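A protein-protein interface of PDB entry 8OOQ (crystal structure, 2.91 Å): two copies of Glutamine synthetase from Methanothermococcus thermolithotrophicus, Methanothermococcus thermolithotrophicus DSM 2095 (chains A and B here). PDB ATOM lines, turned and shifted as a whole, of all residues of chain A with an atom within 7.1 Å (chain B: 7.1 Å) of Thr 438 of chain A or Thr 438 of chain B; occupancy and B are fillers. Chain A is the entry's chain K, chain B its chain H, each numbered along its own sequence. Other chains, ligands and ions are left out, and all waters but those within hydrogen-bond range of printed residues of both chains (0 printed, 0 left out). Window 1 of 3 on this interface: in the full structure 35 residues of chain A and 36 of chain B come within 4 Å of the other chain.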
ATOM      1  N   MET A 237       5.126  29.859 -12.648  1.00  0.00           N
ATOM      2  CA  MET A 237       5.114  30.108 -11.217  1.00  0.00           C
ATOM      3  C   MET A 237       5.427  31.605 -11.019  1.00  0.00           C
ATOM      4  O   MET A 237       6.376  32.096 -11.642  1.00  0.00           O
ATOM      5  CB  MET A 237       6.172  29.231 -10.532  1.00  0.00           C
ATOM      6  CG  MET A 237       6.085  29.226  -9.031  1.00  0.00           C
ATOM      7  SD  MET A 237       7.124  27.932  -8.317  1.00  0.00           S
ATOM      8  CE  MET A 237       7.353  28.557  -6.677  1.00  0.00           C
ATOM      9  N   LYS A 239       7.036  33.277  -8.865  1.00  0.00           N
ATOM     10  CA  LYS A 239       8.363  33.553  -8.305  1.00  0.00           C
ATOM     11  C   LYS A 239       9.063  32.220  -8.011  1.00  0.00           C
ATOM     12  O   LYS A 239       9.077  31.775  -6.863  1.00  0.00           O
ATOM     13  CB  LYS A 239       8.222  34.391  -7.015  1.00  0.00           C
ATOM     14  CG  LYS A 239       9.535  34.904  -6.422  1.00  0.00           C
ATOM     15  CD  LYS A 239      10.024  36.201  -7.056  1.00  0.00           C
ATOM     16  CE  LYS A 239      11.214  36.744  -6.301  1.00  0.00           C
ATOM     17  NZ  LYS A 239      11.693  38.035  -6.852  1.00  0.00           N
ATOM     18  N   PRO A 240       9.582  31.528  -9.041  1.00  0.00           N
ATOM     19  CA  PRO A 240      10.236  30.236  -8.789  1.00  0.00           C
ATOM     20  C   PRO A 240      11.553  30.355  -8.031  1.00  0.00           C
ATOM     21  O   PRO A 240      11.906  29.427  -7.306  1.00  0.00           O
ATOM     22  CB  PRO A 240      10.437  29.657 -10.191  1.00  0.00           C
ATOM     23  CG  PRO A 240      10.493  30.828 -11.078  1.00  0.00           C
ATOM     24  CD  PRO A 240       9.629  31.892 -10.470  1.00  0.00           C
ATOM     25  N   VAL A 298       0.045  31.254  -2.932  1.00  0.00           N
ATOM     26  CA  VAL A 298       0.839  31.736  -1.795  1.00  0.00           C
ATOM     27  C   VAL A 298       2.122  32.396  -2.337  1.00  0.00           C
ATOM     28  O   VAL A 298       2.541  33.437  -1.838  1.00  0.00           O
ATOM     29  CB  VAL A 298       1.179  30.586  -0.810  1.00  0.00           C
ATOM     30  CG1 VAL A 298       2.210  31.029   0.227  1.00  0.00           C
ATOM     31  CG2 VAL A 298      -0.077  30.060  -0.131  1.00  0.00           C
ATOM     32  N   ASN A 299       2.729  31.776  -3.365  1.00  0.00           N
ATOM     33  CA  ASN A 299       3.944  32.262  -4.022  1.00  0.00           C
ATOM     34  C   ASN A 299       3.766  33.620  -4.716  1.00  0.00           C
ATOM     35  O   ASN A 299       4.745  34.347  -4.869  1.00  0.00           O
ATOM     36  CB  ASN A 299       4.437  31.222  -5.023  1.00  0.00           C
ATOM     37  CG  ASN A 299       5.740  31.554  -5.665  1.00  0.00           C
ATOM     38  OD1 ASN A 299       5.810  31.726  -6.871  1.00  0.00           O
ATOM     39  ND2 ASN A 299       6.799  31.648  -4.879  1.00  0.00           N
ATOM     40  N   LYS A 302       5.239  36.650  -2.987  1.00  0.00           N
ATOM     41  CA  LYS A 302       6.700  36.702  -2.899  1.00  0.00           C
ATOM     42  C   LYS A 302       7.220  37.575  -4.080  1.00  0.00           C
ATOM     43  O   LYS A 302       8.271  38.194  -3.942  1.00  0.00           O
ATOM     44  CB  LYS A 302       7.337  35.293  -2.895  1.00  0.00           C
ATOM     45  CG  LYS A 302       7.440  34.639  -1.507  1.00  0.00           C
ATOM     46  CD  LYS A 302       6.103  34.122  -0.983  1.00  0.00           C
ATOM     47  CE  LYS A 302       6.069  33.911   0.512  1.00  0.00           C
ATOM     48  NZ  LYS A 302       7.109  32.961   0.989  1.00  0.00           N
ATOM     49  N   PHE A 433      -0.252  25.699   3.947  1.00  0.00           N
ATOM     50  CA  PHE A 433       0.996  26.457   3.951  1.00  0.00           C
ATOM     51  C   PHE A 433       1.406  26.889   5.367  1.00  0.00           C
ATOM     52  O   PHE A 433       2.562  26.700   5.741  1.00  0.00           O
ATOM     53  CB  PHE A 433       0.880  27.686   3.021  1.00  0.00           C
ATOM     54  CG  PHE A 433       2.023  28.668   3.138  1.00  0.00           C
ATOM     55  CD1 PHE A 433       3.291  28.334   2.704  1.00  0.00           C
ATOM     56  CD2 PHE A 433       1.836  29.907   3.728  1.00  0.00           C
ATOM     57  CE1 PHE A 433       4.342  29.231   2.823  1.00  0.00           C
ATOM     58  CE2 PHE A 433       2.891  30.799   3.851  1.00  0.00           C
ATOM     59  CZ  PHE A 433       4.136  30.458   3.393  1.00  0.00           C
ATOM     60  N   THR A 435       0.667  25.622   8.254  1.00  0.00           N
ATOM     61  CA  THR A 435       0.931  24.500   9.158  1.00  0.00           C
ATOM     62  C   THR A 435       2.222  23.761   8.792  1.00  0.00           C
ATOM     63  O   THR A 435       2.845  23.175   9.674  1.00  0.00           O
ATOM     64  CB  THR A 435      -0.239  23.508   9.148  1.00  0.00           C
ATOM     65  OG1 THR A 435      -0.533  23.130   7.799  1.00  0.00           O
ATOM     66  CG2 THR A 435      -1.480  24.048   9.856  1.00  0.00           C
ATOM     67  N   SER A 436       2.620  23.764   7.507  1.00  0.00           N
ATOM     68  CA  SER A 436       3.821  23.060   7.057  1.00  0.00           C
ATOM     69  C   SER A 436       5.105  23.704   7.560  1.00  0.00           C
ATOM     70  O   SER A 436       5.211  24.930   7.577  1.00  0.00           O
ATOM     71  CB  SER A 436       3.862  22.991   5.532  1.00  0.00           C
ATOM     72  OG  SER A 436       4.122  24.253   4.936  1.00  0.00           O
ATOM     73  N   VAL A 437       6.091  22.876   7.946  1.00  0.00           N
ATOM     74  CA  VAL A 437       7.393  23.352   8.406  1.00  0.00           C
ATOM     75  C   VAL A 437       8.247  23.562   7.155  1.00  0.00           C
ATOM     76  O   VAL A 437       8.569  22.597   6.466  1.00  0.00           O
ATOM     77  CB  VAL A 437       8.041  22.350   9.387  1.00  0.00           C
ATOM     78  CG1 VAL A 437       9.438  22.811   9.791  1.00  0.00           C
ATOM     79  CG2 VAL A 437       7.162  22.159  10.618  1.00  0.00           C
ATOM     80  N   THR A 438       8.586  24.819   6.847  1.00  0.00           N
ATOM     81  CA  THR A 438       9.341  25.174   5.647  1.00  0.00           C
ATOM     82  C   THR A 438      10.858  25.019   5.819  1.00  0.00           C
ATOM     83  O   THR A 438      11.358  24.922   6.939  1.00  0.00           O
ATOM     84  CB  THR A 438       8.974  26.605   5.221  1.00  0.00           C
ATOM     85  OG1 THR A 438       9.437  27.533   6.199  1.00  0.00           O
ATOM     86  CG2 THR A 438       7.477  26.780   4.982  1.00  0.00           C
ATOM     87  N   ASP A 439      11.579  24.974   4.693  1.00  0.00           N
ATOM     88  CA  ASP A 439      13.036  24.875   4.674  1.00  0.00           C
ATOM     89  C   ASP A 439      13.693  26.119   5.285  1.00  0.00           C
ATOM     90  O   ASP A 439      14.773  26.002   5.862  1.00  0.00           O
ATOM     91  CB  ASP A 439      13.554  24.651   3.241  1.00  0.00           C
ATOM     92  CG  ASP A 439      13.227  25.764   2.261  1.00  0.00           C
ATOM     93  OD1 ASP A 439      12.213  26.462   2.470  1.00  0.00           O
ATOM     94  OD2 ASP A 439      13.969  25.918   1.270  1.00  0.00           O
ATOM     95  N   TRP A 440      13.056  27.301   5.157  1.00  0.00           N
ATOM     96  CA  TRP A 440      13.575  28.541   5.735  1.00  0.00           C
ATOM     97  C   TRP A 440      13.609  28.414   7.258  1.00  0.00           C
ATOM     98  O   TRP A 440      14.612  28.772   7.874  1.00  0.00           O
ATOM     99  CB  TRP A 440      12.693  29.737   5.323  1.00  0.00           C
ATOM    100  CG  TRP A 440      13.214  31.071   5.772  1.00  0.00           C
ATOM    101  CD1 TRP A 440      14.008  31.918   5.060  1.00  0.00           C
ATOM    102  CD2 TRP A 440      12.924  31.737   7.007  1.00  0.00           C
ATOM    103  NE1 TRP A 440      14.251  33.061   5.783  1.00  0.00           N
ATOM    104  CE2 TRP A 440      13.607  32.970   6.989  1.00  0.00           C
ATOM    105  CE3 TRP A 440      12.180  31.399   8.144  1.00  0.00           C
ATOM    106  CZ2 TRP A 440      13.558  33.864   8.054  1.00  0.00           C
ATOM    107  CZ3 TRP A 440      12.125  32.292   9.192  1.00  0.00           C
ATOM    108  CH2 TRP A 440      12.811  33.506   9.143  1.00  0.00           C
ATOM    109  N   GLU A 441      12.516  27.905   7.859  1.00  0.00           N
ATOM    110  CA  GLU A 441      12.415  27.714   9.304  1.00  0.00           C
ATOM    111  C   GLU A 441      13.467  26.728   9.794  1.00  0.00           C
ATOM    112  O   GLU A 441      14.079  26.962  10.828  1.00  0.00           O
ATOM    113  CB  GLU A 441      11.029  27.181   9.684  1.00  0.00           C
ATOM    114  CG  GLU A 441       9.899  28.175   9.521  1.00  0.00           C
ATOM    115  CD  GLU A 441       8.549  27.492   9.460  1.00  0.00           C
ATOM    116  OE1 GLU A 441       8.229  26.717  10.390  1.00  0.00           O
ATOM    117  OE2 GLU A 441       7.832  27.688   8.453  1.00  0.00           O
ATOM    118  N   THR A 442      13.674  25.622   9.068  1.00  0.00           N
ATOM    119  CA  THR A 442      14.668  24.625   9.455  1.00  0.00           C
ATOM    120  C   THR A 442      16.068  25.232   9.430  1.00  0.00           C
ATOM    121  O   THR A 442      16.851  24.987  10.339  1.00  0.00           O
ATOM    122  CB  THR A 442      14.553  23.391   8.552  1.00  0.00           C
ATOM    123  OG1 THR A 442      13.206  22.918   8.595  1.00  0.00           O
ATOM    124  CG2 THR A 442      15.507  22.281   8.962  1.00  0.00           C
ATOM    125  N   THR A 443      16.365  26.053   8.421  1.00  0.00           N
ATOM    126  CA  THR A 443      17.668  26.704   8.316  1.00  0.00           C
ATOM    127  C   THR A 443      17.882  27.711   9.451  1.00  0.00           C
ATOM    128  O   THR A 443      18.957  27.744  10.047  1.00  0.00           O
ATOM    129  CB  THR A 443      17.799  27.396   6.951  1.00  0.00           C
ATOM    130  OG1 THR A 443      17.597  26.434   5.914  1.00  0.00           O
ATOM    131  CG2 THR A 443      19.147  28.074   6.769  1.00  0.00           C
ATOM    132  N   MET B 237      13.809  23.676  18.731  1.00  0.00           N
ATOM    133  CA  MET B 237      12.990  24.302  17.703  1.00  0.00           C
ATOM    134  C   MET B 237      11.520  24.022  18.070  1.00  0.00           C
ATOM    135  O   MET B 237      11.201  22.871  18.384  1.00  0.00           O
ATOM    136  CB  MET B 237      13.340  23.702  16.331  1.00  0.00           C
ATOM    137  CG  MET B 237      12.731  24.439  15.168  1.00  0.00           C
ATOM    138  SD  MET B 237      13.447  23.892  13.602  1.00  0.00           S
ATOM    139  CE  MET B 237      12.169  24.373  12.475  1.00  0.00           C
ATOM    140  N   LYS B 239       8.891  23.423  16.416  1.00  0.00           N
ATOM    141  CA  LYS B 239       8.216  22.460  15.538  1.00  0.00           C
ATOM    142  C   LYS B 239       9.188  22.040  14.429  1.00  0.00           C
ATOM    143  O   LYS B 239       9.104  22.555  13.317  1.00  0.00           O
ATOM    144  CB  LYS B 239       6.946  23.100  14.937  1.00  0.00           C
ATOM    145  CG  LYS B 239       6.047  22.149  14.142  1.00  0.00           C
ATOM    146  CD  LYS B 239       5.078  21.357  15.009  1.00  0.00           C
ATOM    147  CE  LYS B 239       4.104  20.587  14.150  1.00  0.00           C
ATOM    148  NZ  LYS B 239       3.108  19.838  14.954  1.00  0.00           N
ATOM    149  N   PRO B 240      10.161  21.164  14.728  1.00  0.00           N
ATOM    150  CA  PRO B 240      11.120  20.763  13.687  1.00  0.00           C
ATOM    151  C   PRO B 240      10.503  19.906  12.590  1.00  0.00           C
ATOM    152  O   PRO B 240      10.978  19.963  11.460  1.00  0.00           O
ATOM    153  CB  PRO B 240      12.195  20.004  14.466  1.00  0.00           C
ATOM    154  CG  PRO B 240      11.508  19.494  15.664  1.00  0.00           C
ATOM    155  CD  PRO B 240      10.424  20.475  16.006  1.00  0.00           C
ATOM    156  N   VAL B 298       9.238  32.413  13.722  1.00  0.00           N
ATOM    157  CA  VAL B 298       8.217  32.168  12.695  1.00  0.00           C
ATOM    158  C   VAL B 298       7.667  30.740  12.880  1.00  0.00           C
ATOM    159  O   VAL B 298       6.465  30.519  12.764  1.00  0.00           O
ATOM    160  CB  VAL B 298       8.788  32.362  11.267  1.00  0.00           C
ATOM    161  CG1 VAL B 298       7.810  31.865  10.203  1.00  0.00           C
ATOM    162  CG2 VAL B 298       9.158  33.820  11.020  1.00  0.00           C
ATOM    163  N   ASN B 299       8.563  29.784  13.174  1.00  0.00           N
ATOM    164  CA  ASN B 299       8.226  28.377  13.403  1.00  0.00           C
ATOM    165  C   ASN B 299       7.323  28.152  14.622  1.00  0.00           C
ATOM    166  O   ASN B 299       6.593  27.164  14.656  1.00  0.00           O
ATOM    167  CB  ASN B 299       9.507  27.558  13.539  1.00  0.00           C
ATOM    168  CG  ASN B 299       9.288  26.084  13.654  1.00  0.00           C
ATOM    169  OD1 ASN B 299       9.626  25.482  14.660  1.00  0.00           O
ATOM    170  ND2 ASN B 299       8.722  25.471  12.629  1.00  0.00           N
ATOM    171  N   LYS B 302       3.669  27.404  13.959  1.00  0.00           N
ATOM    172  CA  LYS B 302       3.374  26.130  13.303  1.00  0.00           C
ATOM    173  C   LYS B 302       3.008  25.094  14.411  1.00  0.00           C
ATOM    174  O   LYS B 302       2.244  24.174  14.134  1.00  0.00           O
ATOM    175  CB  LYS B 302       4.547  25.642  12.420  1.00  0.00           C
ATOM    176  CG  LYS B 302       4.542  26.194  10.984  1.00  0.00           C
ATOM    177  CD  LYS B 302       4.981  27.654  10.898  1.00  0.00           C
ATOM    178  CE  LYS B 302       4.557  28.350   9.624  1.00  0.00           C
ATOM    179  NZ  LYS B 302       5.064  27.679   8.398  1.00  0.00           N
ATOM    180  N   PHE B 433      11.394  36.021   5.940  1.00  0.00           N
ATOM    181  CA  PHE B 433      10.535  34.856   5.746  1.00  0.00           C
ATOM    182  C   PHE B 433       9.499  35.076   4.637  1.00  0.00           C
ATOM    183  O   PHE B 433       9.348  34.211   3.776  1.00  0.00           O
ATOM    184  CB  PHE B 433       9.835  34.480   7.072  1.00  0.00           C
ATOM    185  CG  PHE B 433       8.743  33.447   6.932  1.00  0.00           C
ATOM    186  CD1 PHE B 433       9.045  32.138   6.603  1.00  0.00           C
ATOM    187  CD2 PHE B 433       7.411  33.796   7.080  1.00  0.00           C
ATOM    188  CE1 PHE B 433       8.040  31.192   6.462  1.00  0.00           C
ATOM    189  CE2 PHE B 433       6.409  32.848   6.931  1.00  0.00           C
ATOM    190  CZ  PHE B 433       6.730  31.552   6.627  1.00  0.00           C
ATOM    191  N   THR B 435       9.542  37.078   2.087  1.00  0.00           N
ATOM    192  CA  THR B 435      10.137  37.300   0.767  1.00  0.00           C
ATOM    193  C   THR B 435      10.768  36.023   0.200  1.00  0.00           C
ATOM    194  O   THR B 435      10.840  35.885  -1.017  1.00  0.00           O
ATOM    195  CB  THR B 435      11.199  38.405   0.830  1.00  0.00           C
ATOM    196  OG1 THR B 435      12.139  38.105   1.865  1.00  0.00           O
ATOM    197  CG2 THR B 435      10.599  39.794   1.019  1.00  0.00           C
ATOM    198  N   SER B 436      11.243  35.107   1.061  1.00  0.00           N
ATOM    199  CA  SER B 436      11.892  33.874   0.614  1.00  0.00           C
ATOM    200  C   SER B 436      10.921  32.897  -0.039  1.00  0.00           C
ATOM    201  O   SER B 436       9.801  32.730   0.440  1.00  0.00           O
ATOM    202  CB  SER B 436      12.585  33.178   1.783  1.00  0.00           C
ATOM    203  OG  SER B 436      11.665  32.606   2.700  1.00  0.00           O
ATOM    204  N   VAL B 437      11.365  32.232  -1.119  1.00  0.00           N
ATOM    205  CA  VAL B 437      10.569  31.228  -1.822  1.00  0.00           C
ATOM    206  C   VAL B 437      10.794  29.902  -1.089  1.00  0.00           C
ATOM    207  O   VAL B 437      11.907  29.384  -1.088  1.00  0.00           O
ATOM    208  CB  VAL B 437      10.966  31.141  -3.314  1.00  0.00           C
ATOM    209  CG1 VAL B 437      10.200  30.026  -4.019  1.00  0.00           C
ATOM    210  CG2 VAL B 437      10.735  32.475  -4.012  1.00  0.00           C
ATOM    211  N   THR B 438       9.751  29.379  -0.437  1.00  0.00           N
ATOM    212  CA  THR B 438       9.836  28.158   0.360  1.00  0.00           C
ATOM    213  C   THR B 438       9.704  26.877  -0.477  1.00  0.00           C
ATOM    214  O   THR B 438       9.255  26.918  -1.621  1.00  0.00           O
ATOM    215  CB  THR B 438       8.777  28.206   1.477  1.00  0.00           C
ATOM    216  OG1 THR B 438       7.472  28.144   0.905  1.00  0.00           O
ATOM    217  CG2 THR B 438       8.917  29.441   2.369  1.00  0.00           C
ATOM    218  N   ASP B 439      10.123  25.745   0.102  1.00  0.00           N
ATOM    219  CA  ASP B 439      10.026  24.434  -0.534  1.00  0.00           C
ATOM    220  C   ASP B 439       8.567  24.018  -0.757  1.00  0.00           C
ATOM    221  O   ASP B 439       8.287  23.304  -1.718  1.00  0.00           O
ATOM    222  CB  ASP B 439      10.760  23.365   0.294  1.00  0.00           C
ATOM    223  CG  ASP B 439      10.209  23.156   1.693  1.00  0.00           C
ATOM    224  OD1 ASP B 439       9.634  24.112   2.253  1.00  0.00           O
ATOM    225  OD2 ASP B 439      10.383  22.048   2.240  1.00  0.00           O
ATOM    226  N   TRP B 440       7.645  24.453   0.124  1.00  0.00           N
ATOM    227  CA  TRP B 440       6.221  24.149  -0.017  1.00  0.00           C
ATOM    228  C   TRP B 440       5.690  24.784  -1.303  1.00  0.00           C
ATOM    229  O   TRP B 440       4.977  24.126  -2.060  1.00  0.00           O
ATOM    230  CB  TRP B 440       5.434  24.678   1.198  1.00  0.00           C
ATOM    231  CG  TRP B 440       3.981  24.306   1.200  1.00  0.00           C
ATOM    232  CD1 TRP B 440       3.415  23.219   1.798  1.00  0.00           C
ATOM    233  CD2 TRP B 440       2.900  25.055   0.626  1.00  0.00           C
ATOM    234  NE1 TRP B 440       2.052  23.234   1.615  1.00  0.00           N
ATOM    235  CE2 TRP B 440       1.712  24.347   0.889  1.00  0.00           C
ATOM    236  CE3 TRP B 440       2.825  26.240  -0.116  1.00  0.00           C
ATOM    237  CZ2 TRP B 440       0.466  24.795   0.456  1.00  0.00           C
ATOM    238  CZ3 TRP B 440       1.589  26.682  -0.542  1.00  0.00           C
ATOM    239  CH2 TRP B 440       0.429  25.963  -0.258  1.00  0.00           C
ATOM    240  N   GLU B 441       6.040  26.063  -1.544  1.00  0.00           N
ATOM    241  CA  GLU B 441       5.618  26.793  -2.738  1.00  0.00           C
ATOM    242  C   GLU B 441       6.160  26.130  -3.998  1.00  0.00           C
ATOM    243  O   GLU B 441       5.436  26.012  -4.977  1.00  0.00           O
ATOM    244  CB  GLU B 441       6.118  28.243  -2.693  1.00  0.00           C
ATOM    245  CG  GLU B 441       5.442  29.118  -1.660  1.00  0.00           C
ATOM    246  CD  GLU B 441       6.258  30.354  -1.348  1.00  0.00           C
ATOM    247  OE1 GLU B 441       6.605  31.097  -2.293  1.00  0.00           O
ATOM    248  OE2 GLU B 441       6.602  30.550  -0.160  1.00  0.00           O
ATOM    249  N   THR B 442       7.430  25.708  -3.985  1.00  0.00           N
ATOM    250  CA  THR B 442       8.033  25.053  -5.141  1.00  0.00           C
ATOM    251  C   THR B 442       7.313  23.741  -5.447  1.00  0.00           C
ATOM    252  O   THR B 442       7.048  23.448  -6.608  1.00  0.00           O
ATOM    253  CB  THR B 442       9.534  24.852  -4.909  1.00  0.00           C
ATOM    254  OG1 THR B 442      10.118  26.114  -4.586  1.00  0.00           O
ATOM    255  CG2 THR B 442      10.234  24.250  -6.118  1.00  0.00           C
ATOM    256  N   THR B 443       6.961  22.978  -4.409  1.00  0.00           N
ATOM    257  CA  THR B 443       6.248  21.716  -4.590  1.00  0.00           C
ATOM    258  C   THR B 443       4.839  21.946  -5.150  1.00  0.00           C
ATOM    259  O   THR B 443       4.417  21.237  -6.063  1.00  0.00           O
ATOM    260  CB  THR B 443       6.181  20.959  -3.254  1.00  0.00           C
ATOM    261  OG1 THR B 443       7.506  20.759  -2.759  1.00  0.00           O
ATOM    262  CG2 THR B 443       5.473  19.623  -3.378  1.00  0.00           C
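Of the printed residues of chain B, Thr 438 of chain A touches Phe 433, Thr 438 and Asp 439.
Of the printed residues of chain A, Thr 438 of chain B touches Phe 433, Thr 438 and Asp 439.
Of the printed residues of chain B, Asp 439 of chain A touches Thr 438 (3.6 Å) and Asp 439 (3.2 Å).
Of the printed residues of chain B, Pro 240 of chain A touches Val 437.
Of the printed residues of chain A, Thr 435 of chain B touches Lys 302.
Printed residues of chain A within 4 Å of Ser 436 of chain B: Lys 302 (2.8 Å) and Trp 440 (3.4 Å).
Of the printed residues of chain B, Ser 436 of chain A touches Lys 302 (2.9 Å) and Trp 440 (3.4 Å).
Thr 443 of chain A touches none of the printed residues of chain B.
The nearest printed residue of chain B that does not touch Thr 438 of chain A is Lys 302 of chain B (4.3 Å).
The nearest printed residue of chain A that does not touch Thr 438 of chain B is Lys 302 of chain A (4.2 Å).
The nearest printed residue of chain B that does not touch Thr 442 of chain A is Pro 240 of chain B (4.7 Å).
The side-chain amide oxygen of Asn 299 of chain B sits at hydrogen-bond distance from the backbone NH of Lys 239 of chain B, at 2.8 Å.
O of Phe 433 of chain B sits at hydrogen-bond distance from OG of Ser 436 of chain B, 3.0 Å away.
O of Thr 438 of chain B lies within hydrogen-bond range of OG1 of Thr 442 of chain B (3.2 Å).
The backbone NH (N) of Lys 239 of chain A is in hydrogen-bond range of the side-chain amide oxygen (OD1) of Asn 299 of chain A.
OE2 of Glu 441 of chain A is in hydrogen-bond range of OG1 of Thr 438 of chain A (2.8 Å).
OG1 of Thr 442 of chain A lies within hydrogen-bond range of O of Thr 438 of chain A (3.2 Å).
Of the 16 printed residues of chain A, 15 touch a printed residue of chain B.
Among the printed residues, Asp or Glu carboxylates within 4 Å of a Lys or Arg side-chain nitrogen of the other chain: Lys 302 of chain A with Glu 441 of chain B (2.7 Å) and Glu 441 of chain A with Lys 302 of chain B (2.8 Å).
Met 237 of chain A touches Thr 442 of chain B.
Phe 433 of chain A touches Lys 302 of chain B (O to NZ, 3.8 Å).
Ser 436 of chain A touches Trp 440 of chain B (OG to CD1, 3.4 Å).
Val 437 of chain A touches Lys 239 of chain B.
Val 437 of chain A touches Asn 299 of chain B.
OG1 of Thr 438 of chain A touches CE1 of Phe 433 of chain B, 3.9 Å away.
Asp 439 of chain B touches Thr 438 of chain A (OD1 to CA, 3.6 Å).
Trp 440 of chain A touches Val 298 of chain B (CZ3 to CG2, 3.8 Å).
Trp 440 of chain A touches Phe 433 of chain B.
Trp 440 of chain A touches Ser 436 of chain B.
Lys 239 of chain A touches Val 437 of chain B, and with the chains exchanged Val 437 of chain A touches Lys 239 of chain B.
Lys 302 of chain A touches Ser 436 of chain B, and with the chains exchanged Ser 436 of chain A touches Lys 302 of chain B.
Ser 436 of chain A touches Trp 440 of chain B, and with the chains exchanged Trp 440 of chain A touches Ser 436 of chain B.
Thr 438 of chain B touches its own counterpart, Thr 438 of chain A.
The side-chain carboxylate (OE1) of Glu 441 of chain A is in hydrogen-bond range of the side-chain amide nitrogen (ND2) of Asn 299 of chain B (2.6 Å).
The side-chain amino group (NZ) of Lys 302 of chain B is in hydrogen-bond range of the backbone carbonyl oxygen (O) of Ser 436 of chain A (2.9 Å).
The side-chain carboxylate of Glu 441 of chain A is in salt-bridge range of the side-chain amino group of Lys 302 of chain B (2.8 Å).
NZ of Lys 302 of chain A lies within hydrogen-bond range of O of Ser 436 of chain B, at 2.8 Å.
The side-chain carboxylate (OD1) of Asp 439 of chain B sits at hydrogen-bond distance from the backbone NH (N) of Asp 439 of chain A.
The side-chain amide nitrogen of Asn 299 of chain A sits at hydrogen-bond distance from the side-chain carboxylate of Glu 441 of chain B, at 2.7 Å.
OE2 of Glu 441 of chain B lies within salt-bridge range of NZ of Lys 302 of chain A, 2.7 Å away.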
